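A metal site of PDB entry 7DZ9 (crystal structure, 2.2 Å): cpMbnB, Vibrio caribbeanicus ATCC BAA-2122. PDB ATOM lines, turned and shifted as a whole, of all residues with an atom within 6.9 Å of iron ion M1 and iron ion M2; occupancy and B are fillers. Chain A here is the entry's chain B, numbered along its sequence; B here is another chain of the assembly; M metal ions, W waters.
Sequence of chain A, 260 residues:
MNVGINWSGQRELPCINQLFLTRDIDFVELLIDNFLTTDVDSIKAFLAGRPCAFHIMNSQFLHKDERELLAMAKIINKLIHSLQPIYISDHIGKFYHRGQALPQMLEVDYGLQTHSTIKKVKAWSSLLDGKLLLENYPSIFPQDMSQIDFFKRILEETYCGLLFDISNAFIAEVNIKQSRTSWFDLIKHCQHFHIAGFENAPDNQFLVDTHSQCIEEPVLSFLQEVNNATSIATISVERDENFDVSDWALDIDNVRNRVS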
ATOM      1  N   GLU A  29       5.992 -33.265 -17.423  1.00  0.00           N
ATOM      2  CA  GLU A  29       5.746 -31.934 -16.899  1.00  0.00           C
ATOM      3  C   GLU A  29       7.099 -31.282 -16.626  1.00  0.00           C
ATOM      4  O   GLU A  29       7.777 -31.642 -15.669  1.00  0.00           O
ATOM      5  CB  GLU A  29       4.877 -31.983 -15.646  1.00  0.00           C
ATOM      6  CG  GLU A  29       4.429 -30.595 -15.169  1.00  0.00           C
ATOM      7  CD  GLU A  29       3.851 -30.639 -13.769  1.00  0.00           C
ATOM      8  OE1 GLU A  29       2.597 -30.622 -13.641  1.00  0.00           O
ATOM      9  OE2 GLU A  29       4.654 -30.695 -12.792  1.00  0.00           O
ATOM     10  N   LEU A  31       9.499 -28.484 -15.256  1.00  0.00           N
ATOM     11  CA  LEU A  31       9.613 -27.326 -14.373  1.00  0.00           C
ATOM     12  C   LEU A  31      10.254 -26.240 -15.225  1.00  0.00           C
ATOM     13  O   LEU A  31      11.472 -26.044 -15.242  1.00  0.00           O
ATOM     14  CB  LEU A  31      10.413 -27.666 -13.122  1.00  0.00           C
ATOM     15  CG  LEU A  31      10.123 -26.857 -11.856  1.00  0.00           C
ATOM     16  CD1 LEU A  31       8.652 -26.975 -11.391  1.00  0.00           C
ATOM     17  CD2 LEU A  31      11.075 -27.278 -10.736  1.00  0.00           C
ATOM     18  N   HIS A  55       5.177 -26.462 -15.533  1.00  0.00           N
ATOM     19  CA  HIS A  55       5.014 -26.176 -14.116  1.00  0.00           C
ATOM     20  C   HIS A  55       6.052 -25.131 -13.754  1.00  0.00           C
ATOM     21  O   HIS A  55       7.232 -25.305 -14.066  1.00  0.00           O
ATOM     22  CB  HIS A  55       5.193 -27.469 -13.315  1.00  0.00           C
ATOM     23  CG  HIS A  55       4.698 -27.419 -11.902  1.00  0.00           C
ATOM     24  ND1 HIS A  55       3.486 -26.873 -11.545  1.00  0.00           N
ATOM     25  CD2 HIS A  55       5.256 -27.884 -10.755  1.00  0.00           C
ATOM     26  CE1 HIS A  55       3.317 -26.976 -10.242  1.00  0.00           C
ATOM     27  NE2 HIS A  55       4.375 -27.595  -9.738  1.00  0.00           N
ATOM     28  N   ILE A  56       5.637 -24.026 -13.120  1.00  0.00           N
ATOM     29  CA  ILE A  56       6.536 -22.911 -12.804  1.00  0.00           C
ATOM     30  C   ILE A  56       6.792 -22.894 -11.296  1.00  0.00           C
ATOM     31  O   ILE A  56       5.891 -22.616 -10.513  1.00  0.00           O
ATOM     32  CB  ILE A  56       5.950 -21.568 -13.261  1.00  0.00           C
ATOM     33  CG1 ILE A  56       5.652 -21.598 -14.759  1.00  0.00           C
ATOM     34  CG2 ILE A  56       6.872 -20.424 -12.882  1.00  0.00           C
ATOM     35  CD1 ILE A  56       4.674 -20.514 -15.182  1.00  0.00           C
ATOM     36  N   MET A  57       8.054 -23.082 -10.916  1.00  0.00           N
ATOM     37  CA  MET A  57       8.434 -23.149  -9.515  1.00  0.00           C
ATOM     38  C   MET A  57       8.736 -21.768  -8.925  1.00  0.00           C
ATOM     39  O   MET A  57       8.210 -21.419  -7.874  1.00  0.00           O
ATOM     40  CB  MET A  57       9.661 -24.075  -9.362  1.00  0.00           C
ATOM     41  CG  MET A  57      10.295 -24.110  -7.965  1.00  0.00           C
ATOM     42  SD  MET A  57       9.487 -25.226  -6.827  1.00  0.00           S
ATOM     43  CE  MET A  57       8.187 -24.203  -6.114  1.00  0.00           C
ATOM     44  N   SER A  89       1.173 -23.968 -15.283  1.00  0.00           N
ATOM     45  CA  SER A  89       0.816 -23.996 -13.865  1.00  0.00           C
ATOM     46  C   SER A  89       1.895 -23.297 -13.024  1.00  0.00           C
ATOM     47  O   SER A  89       3.045 -23.214 -13.423  1.00  0.00           O
ATOM     48  CB  SER A  89       0.585 -25.431 -13.384  1.00  0.00           C
ATOM     49  OG  SER A  89       1.771 -26.200 -13.455  1.00  0.00           O
ATOM     50  N   ASP A  90       1.482 -22.787 -11.872  1.00  0.00           N
ATOM     51  CA  ASP A  90       2.389 -22.126 -10.946  1.00  0.00           C
ATOM     52  C   ASP A  90       1.922 -22.452  -9.541  1.00  0.00           C
ATOM     53  O   ASP A  90       0.940 -23.183  -9.335  1.00  0.00           O
ATOM     54  CB  ASP A  90       2.423 -20.607 -11.238  1.00  0.00           C
ATOM     55  CG  ASP A  90       3.708 -19.916 -10.755  1.00  0.00           C
ATOM     56  OD1 ASP A  90       4.258 -20.257  -9.677  1.00  0.00           O
ATOM     57  OD2 ASP A  90       4.144 -18.970 -11.440  1.00  0.00           O
ATOM     58  N   HIS A  91       2.610 -21.885  -8.553  1.00  0.00           N
ATOM     59  CA  HIS A  91       2.339 -22.147  -7.145  1.00  0.00           C
ATOM     60  C   HIS A  91       1.863 -20.879  -6.474  1.00  0.00           C
ATOM     61  O   HIS A  91       2.129 -19.765  -6.938  1.00  0.00           O
ATOM     62  CB  HIS A  91       3.564 -22.643  -6.384  1.00  0.00           C
ATOM     63  CG  HIS A  91       4.162 -23.912  -6.898  1.00  0.00           C
ATOM     64  ND1 HIS A  91       4.972 -23.962  -8.002  1.00  0.00           N
ATOM     65  CD2 HIS A  91       4.080 -25.179  -6.425  1.00  0.00           C
ATOM     66  CE1 HIS A  91       5.360 -25.206  -8.213  1.00  0.00           C
ATOM     67  NE2 HIS A  91       4.833 -25.966  -7.273  1.00  0.00           N
ATOM     68  N   MET A 105      10.214 -22.573  -0.139  1.00  0.00           N
ATOM     69  CA  MET A 105       8.946 -21.917  -0.449  1.00  0.00           C
ATOM     70  C   MET A 105       7.950 -22.194   0.672  1.00  0.00           C
ATOM     71  O   MET A 105       7.605 -23.350   0.956  1.00  0.00           O
ATOM     72  CB  MET A 105       8.390 -22.396  -1.789  1.00  0.00           C
ATOM     73  CG  MET A 105       7.026 -21.769  -2.183  1.00  0.00           C
ATOM     74  SD  MET A 105       6.277 -22.357  -3.753  1.00  0.00           S
ATOM     75  CE  MET A 105       5.312 -23.748  -3.189  1.00  0.00           C
ATOM     76  N   GLU A 135      -1.364 -24.610  -8.047  1.00  0.00           N
ATOM     77  CA  GLU A 135      -1.289 -25.851  -7.284  1.00  0.00           C
ATOM     78  C   GLU A 135      -1.574 -25.604  -5.806  1.00  0.00           C
ATOM     79  O   GLU A 135      -1.110 -24.622  -5.239  1.00  0.00           O
ATOM     80  CB  GLU A 135       0.092 -26.476  -7.455  1.00  0.00           C
ATOM     81  CG  GLU A 135       0.231 -27.833  -6.778  1.00  0.00           C
ATOM     82  CD  GLU A 135       1.611 -28.445  -6.955  1.00  0.00           C
ATOM     83  OE1 GLU A 135       2.562 -27.725  -7.337  1.00  0.00           O
ATOM     84  OE2 GLU A 135       1.755 -29.663  -6.713  1.00  0.00           O
ATOM     85  N   ASN A 136      -2.335 -26.501  -5.183  1.00  0.00           N
ATOM     86  CA  ASN A 136      -2.544 -26.446  -3.737  1.00  0.00           C
ATOM     87  C   ASN A 136      -1.263 -26.771  -2.982  1.00  0.00           C
ATOM     88  O   ASN A 136      -0.482 -27.639  -3.396  1.00  0.00           O
ATOM     89  CB  ASN A 136      -3.674 -27.393  -3.289  1.00  0.00           C
ATOM     90  CG  ASN A 136      -3.503 -28.810  -3.797  1.00  0.00           C
ATOM     91  OD1 ASN A 136      -3.443 -29.051  -5.006  1.00  0.00           O
ATOM     92  ND2 ASN A 136      -3.443 -29.766  -2.872  1.00  0.00           N
ATOM     93  N   LEU A 163      -4.679 -26.891 -10.339  1.00  0.00           N
ATOM     94  CA  LEU A 163      -3.894 -28.113 -10.531  1.00  0.00           C
ATOM     95  C   LEU A 163      -3.890 -28.815  -9.173  1.00  0.00           C
ATOM     96  O   LEU A 163      -3.308 -28.295  -8.213  1.00  0.00           O
ATOM     97  CB  LEU A 163      -2.473 -27.793 -11.004  1.00  0.00           C
ATOM     98  CG  LEU A 163      -1.447 -28.939 -11.018  1.00  0.00           C
ATOM     99  CD1 LEU A 163      -1.781 -29.993 -12.078  1.00  0.00           C
ATOM    100  CD2 LEU A 163      -0.020 -28.427 -11.266  1.00  0.00           C
ATOM    101  N   PHE A 164      -4.579 -29.939  -9.067  1.00  0.00           N
ATOM    102  CA  PHE A 164      -4.829 -30.506  -7.742  1.00  0.00           C
ATOM    103  C   PHE A 164      -3.760 -31.529  -7.424  1.00  0.00           C
ATOM    104  O   PHE A 164      -3.623 -32.518  -8.136  1.00  0.00           O
ATOM    105  CB  PHE A 164      -6.209 -31.164  -7.631  1.00  0.00           C
ATOM    106  CG  PHE A 164      -6.515 -31.664  -6.237  1.00  0.00           C
ATOM    107  CD1 PHE A 164      -6.643 -30.775  -5.183  1.00  0.00           C
ATOM    108  CD2 PHE A 164      -6.671 -33.024  -5.995  1.00  0.00           C
ATOM    109  CE1 PHE A 164      -6.920 -31.218  -3.880  1.00  0.00           C
ATOM    110  CE2 PHE A 164      -6.954 -33.496  -4.699  1.00  0.00           C
ATOM    111  CZ  PHE A 164      -7.075 -32.591  -3.631  1.00  0.00           C
ATOM    112  N   ASP A 165      -2.992 -31.276  -6.355  1.00  0.00           N
ATOM    113  CA  ASP A 165      -1.975 -32.210  -5.902  1.00  0.00           C
ATOM    114  C   ASP A 165      -2.581 -33.094  -4.810  1.00  0.00           C
ATOM    115  O   ASP A 165      -2.824 -32.635  -3.682  1.00  0.00           O
ATOM    116  CB  ASP A 165      -0.719 -31.486  -5.415  1.00  0.00           C
ATOM    117  CG  ASP A 165       0.445 -32.432  -5.247  1.00  0.00           C
ATOM    118  OD1 ASP A 165       0.299 -33.407  -4.476  1.00  0.00           O
ATOM    119  OD2 ASP A 165       1.515 -32.219  -5.854  1.00  0.00           O
ATOM    120  N   ILE A 166      -2.773 -34.372  -5.141  1.00  0.00           N
ATOM    121  CA  ILE A 166      -3.489 -35.296  -4.252  1.00  0.00           C
ATOM    122  C   ILE A 166      -2.691 -35.545  -2.982  1.00  0.00           C
ATOM    123  O   ILE A 166      -3.242 -35.592  -1.880  1.00  0.00           O
ATOM    124  CB  ILE A 166      -3.802 -36.603  -4.998  1.00  0.00           C
ATOM    125  CG1 ILE A 166      -4.698 -36.310  -6.208  1.00  0.00           C
ATOM    126  CG2 ILE A 166      -4.455 -37.623  -4.057  1.00  0.00           C
ATOM    127  CD1 ILE A 166      -4.746 -37.481  -7.178  1.00  0.00           C
ATOM    128  N   SER A 167      -1.373 -35.718  -3.106  1.00  0.00           N
ATOM    129  CA  SER A 167      -0.613 -35.997  -1.898  1.00  0.00           C
ATOM    130  C   SER A 167      -0.350 -34.734  -1.080  1.00  0.00           C
ATOM    131  O   SER A 167      -0.255 -34.810   0.153  1.00  0.00           O
ATOM    132  CB  SER A 167       0.698 -36.716  -2.243  1.00  0.00           C
ATOM    133  OG  SER A 167       1.476 -35.970  -3.138  1.00  0.00           O
ATOM    134  N   ASN A 168      -0.233 -33.569  -1.738  1.00  0.00           N
ATOM    135  CA  ASN A 168      -0.193 -32.312  -0.977  1.00  0.00           C
ATOM    136  C   ASN A 168      -1.431 -32.159  -0.099  1.00  0.00           C
ATOM    137  O   ASN A 168      -1.337 -31.733   1.058  1.00  0.00           O
ATOM    138  CB  ASN A 168      -0.056 -31.112  -1.908  1.00  0.00           C
ATOM    139  CG  ASN A 168       1.297 -31.047  -2.614  1.00  0.00           C
ATOM    140  OD1 ASN A 168       2.087 -31.972  -2.537  1.00  0.00           O
ATOM    141  ND2 ASN A 168       1.535 -29.960  -3.325  1.00  0.00           N
ATOM    142  N   HIS A 194      -1.493 -34.027  -9.662  1.00  0.00           N
ATOM    143  CA  HIS A 194      -0.208 -34.504  -9.178  1.00  0.00           C
ATOM    144  C   HIS A 194      -0.447 -35.560  -8.105  1.00  0.00           C
ATOM    145  O   HIS A 194      -1.442 -35.517  -7.382  1.00  0.00           O
ATOM    146  CB  HIS A 194       0.618 -33.392  -8.524  1.00  0.00           C
ATOM    147  CG  HIS A 194       1.259 -32.446  -9.481  1.00  0.00           C
ATOM    148  ND1 HIS A 194       2.176 -31.497  -9.072  1.00  0.00           N
ATOM    149  CD2 HIS A 194       1.126 -32.285 -10.817  1.00  0.00           C
ATOM    150  CE1 HIS A 194       2.586 -30.804 -10.119  1.00  0.00           C
ATOM    151  NE2 HIS A 194       1.946 -31.251 -11.187  1.00  0.00           N
ATOM    152  N   ILE A 195       0.530 -36.469  -7.964  1.00  0.00           N
ATOM    153  CA  ILE A 195       0.571 -37.431  -6.874  1.00  0.00           C
ATOM    154  C   ILE A 195       2.030 -37.818  -6.642  1.00  0.00           C
ATOM    155  O   ILE A 195       2.808 -37.919  -7.601  1.00  0.00           O
ATOM    156  CB  ILE A 195      -0.316 -38.668  -7.191  1.00  0.00           C
ATOM    157  CG1 ILE A 195      -0.618 -39.472  -5.936  1.00  0.00           C
ATOM    158  CG2 ILE A 195       0.297 -39.525  -8.293  1.00  0.00           C
ATOM    159  CD1 ILE A 195      -1.635 -40.574  -6.199  1.00  0.00           C
ATOM    160  N   ALA A 196       2.414 -37.986  -5.379  1.00  0.00           N
ATOM    161  CA  ALA A 196       3.823 -38.199  -5.048  1.00  0.00           C
ATOM    162  C   ALA A 196       3.954 -38.803  -3.647  1.00  0.00           C
ATOM    163  O   ALA A 196       2.980 -38.928  -2.909  1.00  0.00           O
ATOM    164  CB  ALA A 196       4.606 -36.894  -5.133  1.00  0.00           C
ATOM    165  N   ASP A 209       6.770 -32.660   2.175  1.00  0.00           N
ATOM    166  CA  ASP A 209       6.397 -32.965   0.788  1.00  0.00           C
ATOM    167  C   ASP A 209       7.680 -33.123  -0.043  1.00  0.00           C
ATOM    168  O   ASP A 209       8.035 -32.276  -0.852  1.00  0.00           O
ATOM    169  CB  ASP A 209       5.488 -31.855   0.244  1.00  0.00           C
ATOM    170  CG  ASP A 209       5.046 -32.105  -1.194  1.00  0.00           C
ATOM    171  OD1 ASP A 209       4.729 -33.258  -1.533  1.00  0.00           O
ATOM    172  OD2 ASP A 209       4.993 -31.118  -1.976  1.00  0.00           O
ATOM    173  N   HIS A 211       8.627 -35.586  -2.286  1.00  0.00           N
ATOM    174  CA  HIS A 211       8.620 -36.279  -3.583  1.00  0.00           C
ATOM    175  C   HIS A 211       9.793 -37.262  -3.671  1.00  0.00           C
ATOM    176  O   HIS A 211      10.467 -37.381  -4.708  1.00  0.00           O
ATOM    177  CB  HIS A 211       8.687 -35.292  -4.759  1.00  0.00           C
ATOM    178  CG  HIS A 211       7.614 -34.240  -4.748  1.00  0.00           C
ATOM    179  ND1 HIS A 211       7.691 -33.094  -5.510  1.00  0.00           N
ATOM    180  CD2 HIS A 211       6.423 -34.172  -4.089  1.00  0.00           C
ATOM    181  CE1 HIS A 211       6.613 -32.353  -5.301  1.00  0.00           C
ATOM    182  NE2 HIS A 211       5.834 -32.985  -4.447  1.00  0.00           N
ATOM    183  N   SER A 236       0.581 -36.292 -13.010  1.00  0.00           N
ATOM    184  CA  SER A 236       2.022 -36.359 -13.003  1.00  0.00           C
ATOM    185  C   SER A 236       2.462 -37.047 -11.704  1.00  0.00           C
ATOM    186  O   SER A 236       2.077 -36.617 -10.611  1.00  0.00           O
ATOM    187  CB  SER A 236       2.630 -34.952 -13.116  1.00  0.00           C
ATOM    188  OG  SER A 236       4.015 -34.946 -12.826  1.00  0.00           O
ATOM    189  N   GLU A 238       5.221 -37.473  -9.351  1.00  0.00           N
ATOM    190  CA  GLU A 238       6.401 -36.646  -9.136  1.00  0.00           C
ATOM    191  C   GLU A 238       7.500 -37.390  -8.380  1.00  0.00           C
ATOM    192  O   GLU A 238       7.227 -38.181  -7.467  1.00  0.00           O
ATOM    193  CB  GLU A 238       6.051 -35.374  -8.369  1.00  0.00           C
ATOM    194  CG  GLU A 238       4.693 -34.761  -8.674  1.00  0.00           C
ATOM    195  CD  GLU A 238       4.589 -33.356  -8.094  1.00  0.00           C
ATOM    196  OE1 GLU A 238       3.955 -33.167  -7.052  1.00  0.00           O
ATOM    197  OE2 GLU A 238       5.204 -32.447  -8.662  1.00  0.00           O
ATOM    198  N   THR B  17      13.641 -27.634  -7.016  1.00  0.00           N
ATOM    199  CA  THR B  17      12.662 -28.679  -7.197  1.00  0.00           C
ATOM    200  C   THR B  17      11.428 -28.328  -6.373  1.00  0.00           C
ATOM    201  O   THR B  17      11.481 -27.455  -5.500  1.00  0.00           O
ATOM    202  CB  THR B  17      13.198 -30.067  -6.770  1.00  0.00           C
ATOM    203  OG1 THR B  17      13.664 -30.016  -5.415  1.00  0.00           O
ATOM    204  CG2 THR B  17      14.367 -30.510  -7.677  1.00  0.00           C
ATOM    205  N   CYS B  18      10.308 -28.992  -6.682  1.00  0.00           N
ATOM    206  CA  CYS B  18       9.129 -28.790  -5.857  1.00  0.00           C
ATOM    207  C   CYS B  18       9.274 -29.536  -4.537  1.00  0.00           C
ATOM    208  O   CYS B  18       8.687 -29.137  -3.534  1.00  0.00           O
ATOM    209  CB  CYS B  18       7.875 -29.313  -6.550  1.00  0.00           C
ATOM    210  SG  CYS B  18       7.205 -28.260  -7.793  1.00  0.00           S
ATOM    211  N   GLY B  19      10.072 -30.592  -4.535  1.00  0.00           N
ATOM    212  CA  GLY B  19      10.346 -31.360  -3.345  1.00  0.00           C
ATOM    213  C   GLY B  19      10.947 -30.543  -2.220  1.00  0.00           C
ATOM    214  O   GLY B  19      11.999 -29.907  -2.386  1.00  0.00           O
HETATM  215 FE    FE M   1       2.984 -31.208  -6.912  1.00  0.00          FE
HETATM  216 FE    FE M   2       4.681 -28.111  -7.577  1.00  0.00          FE
HETATM  217 FE    FE M   3       3.994 -32.257  -3.571  1.00  0.00          FE
HETATM  218  O   HOH W   1       4.844 -28.186  -5.292  1.00  0.00           O
HETATM  219  O   HOH W   2       3.622 -30.679  -5.087  1.00  0.00           O
HETATM  220  O   HOH W   3       4.507 -30.004  -7.632  1.00  0.00           O
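Four residues have an atom within 4 Å of iron ion M2: His 55, His 91, Glu 135 and Cys 18 of chain B. The nearest printed residue that does not touch iron ion M2 is His 194 (4.3 Å).
Iron ion M1 is bound by OE2 of Glu 135, at 2.0 Å. Iron ion M1 is bound by water W2 (2.0 Å). Iron ion M1 is bound by water W3 (2.1 Å). OD2 of Asp 165 is bound to iron ion M1 (2.1 Å). The side-chain carboxylate (OE1) of Glu 238 is bound to iron ion M1. Iron ion M1 is bound by ND1 of His 194 (2.3 Å).
Iron ion M2 is bound by water W3, OE1 of Glu 135, NE2 of His 91, NE2 of His 55, water W1 and SG of Cys 18 of chain B. Iron ion M2 has six donor atoms within binding distance.
The nearest printed residue that does not touch iron ion M1 is Asn 168 (4.1 Å).
OG of Ser 167 is in hydrogen-bond range of OD1 of Asp 165 (3.1 Å). ND1 of His 91 sits at hydrogen-bond distance from O of Ile 56, 3.0 Å away. The side-chain amide nitrogen (ND2) of Asn 168 sits close to the side-chain carboxylate (OE2) of Glu 135, at 3.4 Å. The backbone carbonyl oxygen of Asp 90 lies within hydrogen-bond range of the backbone NH of Glu 135 (3.0 Å). The backbone NH of Ile 166 lies within hydrogen-bond range of the backbone carbonyl oxygen of His 194. The backbone NH (N) of Glu 238 is in hydrogen-bond range of the backbone carbonyl oxygen (O) of Ile 195 (3.0 Å). The backbone NH (N) of Asp 165 lies within hydrogen-bond range of the side-chain amide oxygen (OD1) of Asn 136 (2.6 Å). The side-chain carboxylate of Glu 29 sits at hydrogen-bond distance from a ring nitrogen (NE2) of His 194, at 2.6 Å.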
